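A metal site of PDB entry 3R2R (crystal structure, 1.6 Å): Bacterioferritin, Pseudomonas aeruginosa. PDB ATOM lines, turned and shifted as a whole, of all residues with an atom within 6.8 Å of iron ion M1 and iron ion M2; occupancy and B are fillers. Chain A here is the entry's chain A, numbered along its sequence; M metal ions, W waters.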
ATOM      1  N   GLY A  17     -16.642  10.955  29.530  1.00  0.00           N
ATOM      2  CA  GLY A  17     -15.586  10.344  28.720  1.00  0.00           C
ATOM      3  C   GLY A  17     -16.193   9.423  27.650  1.00  0.00           C
ATOM      4  O   GLY A  17     -15.743   9.374  26.515  1.00  0.00           O
ATOM      5  N   GLU A  18     -17.212   8.639  28.011  1.00  0.00           N
ATOM      6  CA  GLU A  18     -17.816   7.715  27.034  1.00  0.00           C
ATOM      7  C   GLU A  18     -18.659   8.443  25.975  1.00  0.00           C
ATOM      8  O   GLU A  18     -18.672   8.056  24.797  1.00  0.00           O
ATOM      9  CB  GLU A  18     -18.691   6.665  27.732  1.00  0.00           C
ATOM     10  CG  GLU A  18     -17.900   5.805  28.707  1.00  0.00           C
ATOM     11  CD  GLU A  18     -16.778   5.049  28.011  1.00  0.00           C
ATOM     12  OE1 GLU A  18     -17.042   4.444  26.954  1.00  0.00           O
ATOM     13  OE2 GLU A  18     -15.659   5.049  28.577  1.00  0.00           O
ATOM     14  N   ALA A  21     -16.108   9.621  23.571  1.00  0.00           N
ATOM     15  CA  ALA A  21     -15.608   8.527  22.690  1.00  0.00           C
ATOM     16  C   ALA A  21     -16.644   8.272  21.575  1.00  0.00           C
ATOM     17  O   ALA A  21     -16.284   8.185  20.395  1.00  0.00           O
ATOM     18  CB  ALA A  21     -15.351   7.268  23.521  1.00  0.00           C
ATOM     19  N   TYR A  25     -15.852   8.927  17.541  1.00  0.00           N
ATOM     20  CA  TYR A  25     -16.062   7.896  16.514  1.00  0.00           C
ATOM     21  C   TYR A  25     -17.157   8.306  15.498  1.00  0.00           C
ATOM     22  O   TYR A  25     -17.117   7.908  14.310  1.00  0.00           O
ATOM     23  CB  TYR A  25     -16.426   6.562  17.181  1.00  0.00           C
ATOM     24  CG  TYR A  25     -15.252   5.969  17.927  1.00  0.00           C
ATOM     25  CD1 TYR A  25     -13.979   6.011  17.377  1.00  0.00           C
ATOM     26  CD2 TYR A  25     -15.418   5.326  19.130  1.00  0.00           C
ATOM     27  CE1 TYR A  25     -12.885   5.433  18.030  1.00  0.00           C
ATOM     28  CE2 TYR A  25     -14.324   4.758  19.818  1.00  0.00           C
ATOM     29  CZ  TYR A  25     -13.074   4.835  19.253  1.00  0.00           C
ATOM     30  OH  TYR A  25     -11.997   4.263  19.892  1.00  0.00           O
ATOM     31  N   GLU A  47     -17.985   0.994  16.465  1.00  0.00           N
ATOM     32  CA  GLU A  47     -17.444   1.440  17.752  1.00  0.00           C
ATOM     33  C   GLU A  47     -18.303   2.577  18.335  1.00  0.00           C
ATOM     34  O   GLU A  47     -18.459   2.661  19.546  1.00  0.00           O
ATOM     35  CB  GLU A  47     -16.014   1.970  17.595  1.00  0.00           C
ATOM     36  CG  GLU A  47     -15.110   1.073  16.753  1.00  0.00           C
ATOM     37  CD  GLU A  47     -14.707  -0.170  17.455  1.00  0.00           C
ATOM     38  OE1 GLU A  47     -13.475  -0.377  17.643  1.00  0.00           O
ATOM     39  OE2 GLU A  47     -15.600  -0.980  17.778  1.00  0.00           O
ATOM     40  N   GLU A  50     -20.976   0.947  20.076  1.00  0.00           N
ATOM     41  CA  GLU A  50     -20.459   0.360  21.310  1.00  0.00           C
ATOM     42  C   GLU A  50     -20.209   1.385  22.419  1.00  0.00           C
ATOM     43  O   GLU A  50     -20.549   1.130  23.577  1.00  0.00           O
ATOM     44  CB  GLU A  50     -19.200  -0.426  21.038  1.00  0.00           C
ATOM     45  CG  GLU A  50     -19.593  -1.690  20.234  1.00  0.00           C
ATOM     46  CD  GLU A  50     -18.435  -2.600  19.982  1.00  0.00           C
ATOM     47  OE1 GLU A  50     -18.664  -3.828  19.901  1.00  0.00           O
ATOM     48  OE2 GLU A  50     -17.304  -2.098  19.827  1.00  0.00           O
ATOM     49  N   GLU A  51     -19.700   2.566  22.065  1.00  0.00           N
ATOM     50  CA  GLU A  51     -19.494   3.571  23.115  1.00  0.00           C
ATOM     51  C   GLU A  51     -20.845   4.106  23.595  1.00  0.00           C
ATOM     52  O   GLU A  51     -20.984   4.526  24.748  1.00  0.00           O
ATOM     53  CB  GLU A  51     -18.653   4.763  22.601  1.00  0.00           C
ATOM     54  CG  GLU A  51     -17.279   4.339  22.081  1.00  0.00           C
ATOM     55  CD  GLU A  51     -16.370   3.781  23.148  1.00  0.00           C
ATOM     56  OE1 GLU A  51     -16.791   3.575  24.267  1.00  0.00           O
ATOM     57  OE2 GLU A  51     -15.246   3.446  22.801  1.00  0.00           O
ATOM     58  N   HIS A  54     -21.767   1.772  26.159  1.00  0.00           N
ATOM     59  CA  HIS A  54     -20.955   1.998  27.383  1.00  0.00           C
ATOM     60  C   HIS A  54     -21.513   3.186  28.161  1.00  0.00           C
ATOM     61  O   HIS A  54     -21.650   3.117  29.370  1.00  0.00           O
ATOM     62  CB  HIS A  54     -19.514   2.315  27.015  1.00  0.00           C
ATOM     63  CG  HIS A  54     -18.712   1.110  26.650  1.00  0.00           C
ATOM     64  ND1 HIS A  54     -17.388   1.187  26.278  1.00  0.00           N
ATOM     65  CD2 HIS A  54     -19.053  -0.199  26.600  1.00  0.00           C
ATOM     66  CE1 HIS A  54     -16.937  -0.033  26.011  1.00  0.00           C
ATOM     67  NE2 HIS A  54     -17.924  -0.893  26.211  1.00  0.00           N
ATOM     68  N   ALA A  55     -21.795   4.279  27.453  1.00  0.00           N
ATOM     69  CA  ALA A  55     -22.370   5.445  28.099  1.00  0.00           C
ATOM     70  C   ALA A  55     -23.704   5.092  28.752  1.00  0.00           C
ATOM     71  O   ALA A  55     -23.994   5.505  29.878  1.00  0.00           O
ATOM     72  CB  ALA A  55     -22.540   6.652  27.094  1.00  0.00           C
ATOM     73  N   LEU A  92      -7.231   8.329  22.910  1.00  0.00           N
ATOM     74  CA  LEU A  92      -8.525   8.353  23.577  1.00  0.00           C
ATOM     75  C   LEU A  92      -8.766   7.054  24.351  1.00  0.00           C
ATOM     76  O   LEU A  92      -9.162   7.053  25.500  1.00  0.00           O
ATOM     77  CB  LEU A  92      -9.631   8.550  22.516  1.00  0.00           C
ATOM     78  CG  LEU A  92     -11.065   8.618  23.036  1.00  0.00           C
ATOM     79  CD1 LEU A  92     -11.164   9.508  24.260  1.00  0.00           C
ATOM     80  CD2 LEU A  92     -11.968   9.139  21.936  1.00  0.00           C
ATOM     81  N   GLU A  93      -8.564   5.923  23.686  1.00  0.00           N
ATOM     82  CA  GLU A  93      -8.780   4.635  24.357  1.00  0.00           C
ATOM     83  C   GLU A  93      -7.801   4.416  25.503  1.00  0.00           C
ATOM     84  O   GLU A  93      -8.192   3.872  26.512  1.00  0.00           O
ATOM     85  CB  GLU A  93      -8.749   3.476  23.355  1.00  0.00           C
ATOM     86  CG  GLU A  93      -9.939   3.535  22.363  1.00  0.00           C
ATOM     87  CD  GLU A  93     -11.278   3.121  22.972  1.00  0.00           C
ATOM     88  OE1 GLU A  93     -11.315   2.417  24.011  1.00  0.00           O
ATOM     89  OE2 GLU A  93     -12.324   3.490  22.382  1.00  0.00           O
ATOM     90  N   VAL A  96      -9.271   6.418  28.357  1.00  0.00           N
ATOM     91  CA  VAL A  96     -10.398   5.668  28.918  1.00  0.00           C
ATOM     92  C   VAL A  96      -9.935   4.481  29.780  1.00  0.00           C
ATOM     93  O   VAL A  96     -10.454   4.243  30.889  1.00  0.00           O
ATOM     94  CB  VAL A  96     -11.303   5.161  27.783  1.00  0.00           C
ATOM     95  CG1 VAL A  96     -12.376   4.170  28.309  1.00  0.00           C
ATOM     96  CG2 VAL A  96     -11.968   6.349  27.068  1.00  0.00           C
ATOM     97  N   LEU A 100     -10.917   4.102  33.610  1.00  0.00           N
ATOM     98  CA  LEU A 100     -11.680   2.931  34.108  1.00  0.00           C
ATOM     99  C   LEU A 100     -10.935   2.189  35.241  1.00  0.00           C
ATOM    100  O   LEU A 100     -11.512   1.823  36.245  1.00  0.00           O
ATOM    101  CB  LEU A 100     -11.954   1.957  32.954  1.00  0.00           C
ATOM    102  CG  LEU A 100     -13.013   2.430  31.951  1.00  0.00           C
ATOM    103  CD1 LEU A 100     -12.940   1.484  30.727  1.00  0.00           C
ATOM    104  CD2 LEU A 100     -14.417   2.396  32.598  1.00  0.00           C
ATOM    105  N   GLN A 122     -16.396  -2.896  30.714  1.00  0.00           N
ATOM    106  CA  GLN A 122     -15.954  -1.887  29.754  1.00  0.00           C
ATOM    107  C   GLN A 122     -14.436  -1.854  29.581  1.00  0.00           C
ATOM    108  O   GLN A 122     -13.931  -1.566  28.490  1.00  0.00           O
ATOM    109  CB  GLN A 122     -16.428  -0.487  30.185  1.00  0.00           C
ATOM    110  CG  GLN A 122     -17.910  -0.420  30.204  1.00  0.00           C
ATOM    111  CD  GLN A 122     -18.438   0.992  30.219  1.00  0.00           C
ATOM    112  OE1 GLN A 122     -17.726   1.974  29.899  1.00  0.00           O
ATOM    113  NE2 GLN A 122     -19.707   1.111  30.555  1.00  0.00           N
ATOM    114  N   ASP A 125     -13.529  -4.480  27.096  1.00  0.00           N
ATOM    115  CA  ASP A 125     -13.854  -3.973  25.743  1.00  0.00           C
ATOM    116  C   ASP A 125     -12.801  -2.992  25.277  1.00  0.00           C
ATOM    117  O   ASP A 125     -12.314  -3.069  24.126  1.00  0.00           O
ATOM    118  CB  ASP A 125     -15.217  -3.265  25.696  1.00  0.00           C
ATOM    119  CG  ASP A 125     -16.421  -4.211  25.903  1.00  0.00           C
ATOM    120  OD1 ASP A 125     -16.261  -5.458  25.773  1.00  0.00           O
ATOM    121  OD2 ASP A 125     -17.522  -3.692  26.183  1.00  0.00           O
ATOM    122  N   THR A 126     -12.441  -2.074  26.157  1.00  0.00           N
ATOM    123  CA  THR A 126     -11.450  -1.036  25.813  1.00  0.00           C
ATOM    124  C   THR A 126     -10.092  -1.652  25.460  1.00  0.00           C
ATOM    125  O   THR A 126      -9.489  -1.313  24.449  1.00  0.00           O
ATOM    126  CB  THR A 126     -11.324  -0.041  26.999  1.00  0.00           C
ATOM    127  OG1 THR A 126     -12.608   0.574  27.210  1.00  0.00           O
ATOM    128  CG2 THR A 126     -10.284   1.019  26.685  1.00  0.00           C
ATOM    129  N   HIS A 130     -11.269  -2.356  21.446  1.00  0.00           N
ATOM    130  CA  HIS A 130     -11.127  -0.994  20.890  1.00  0.00           C
ATOM    131  C   HIS A 130      -9.681  -0.562  20.690  1.00  0.00           C
ATOM    132  O   HIS A 130      -9.267  -0.205  19.567  1.00  0.00           O
ATOM    133  CB  HIS A 130     -11.808   0.036  21.786  1.00  0.00           C
ATOM    134  CG  HIS A 130     -13.283  -0.138  21.852  1.00  0.00           C
ATOM    135  ND1 HIS A 130     -14.099   0.653  22.631  1.00  0.00           N
ATOM    136  CD2 HIS A 130     -14.104  -1.008  21.211  1.00  0.00           C
ATOM    137  CE1 HIS A 130     -15.359   0.279  22.488  1.00  0.00           C
ATOM    138  NE2 HIS A 130     -15.393  -0.735  21.622  1.00  0.00           N
ATOM    139  N   ALA A 131      -8.914  -0.531  21.778  1.00  0.00           N
ATOM    140  CA  ALA A 131      -7.515  -0.140  21.657  1.00  0.00           C
ATOM    141  C   ALA A 131      -6.747  -1.167  20.810  1.00  0.00           C
ATOM    142  O   ALA A 131      -5.896  -0.798  20.022  1.00  0.00           O
ATOM    143  CB  ALA A 131      -6.857   0.008  23.037  1.00  0.00           C
HETATM  144 FE    FE M   1     -16.038   2.869  26.174  1.00  0.00          FE
HETATM  145 FE    FE M   2     -13.667   2.528  23.672  1.00  0.00          FE
HETATM  146  O   HOH W   1     -14.208   2.193  25.540  1.00  0.00           O
HETATM  147  O   HOH W   2     -15.460   2.369  28.272  1.00  0.00           O
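Iron ion M2 is bound by water W1, the side-chain carboxylate (OE2) of Glu 51, the side-chain carboxylate (OE2) of Glu 93, a ring nitrogen (ND1) of His 130 and the side-chain carboxylate (OE1) of Glu 93.
The side-chain carboxylate (OE2) of Glu 93 sits close to the side-chain hydroxyl (OH) of Tyr 25 (2.6 Å). The side-chain amide nitrogen of Gln 122 is in hydrogen-bond range of the backbone carbonyl oxygen of His 54, at 3.0 Å. NE2 of His 54 is in hydrogen-bond range of OD2 of Asp 125, at 2.8 Å. NE2 of His 130 is in hydrogen-bond range of OE2 of Glu 50, 3.0 Å away. The backbone carbonyl oxygen (O) of Asp 125 is in hydrogen-bond range of the backbone NH (N) of His 130 (3.0 Å).
Of the 18 residues printed, 3 come within 4 Å of iron ion M1.
Water W2 lies within hydrogen-bond range of the side-chain carboxylate of Glu 18 and the side-chain amide oxygen of Gln 122.
Within 4 Å of iron ion M2: Glu 51, Glu 93 and His 130.
Iron ion M1 is bound by OE1 of Glu 18 (2.0 Å), water W1 (2.1 Å), ND1 of His 54 (2.2 Å), OE1 of Glu 51 (2.2 Å) and water W2 (2.2 Å). Iron ion M1 has five donor atoms within binding distance.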
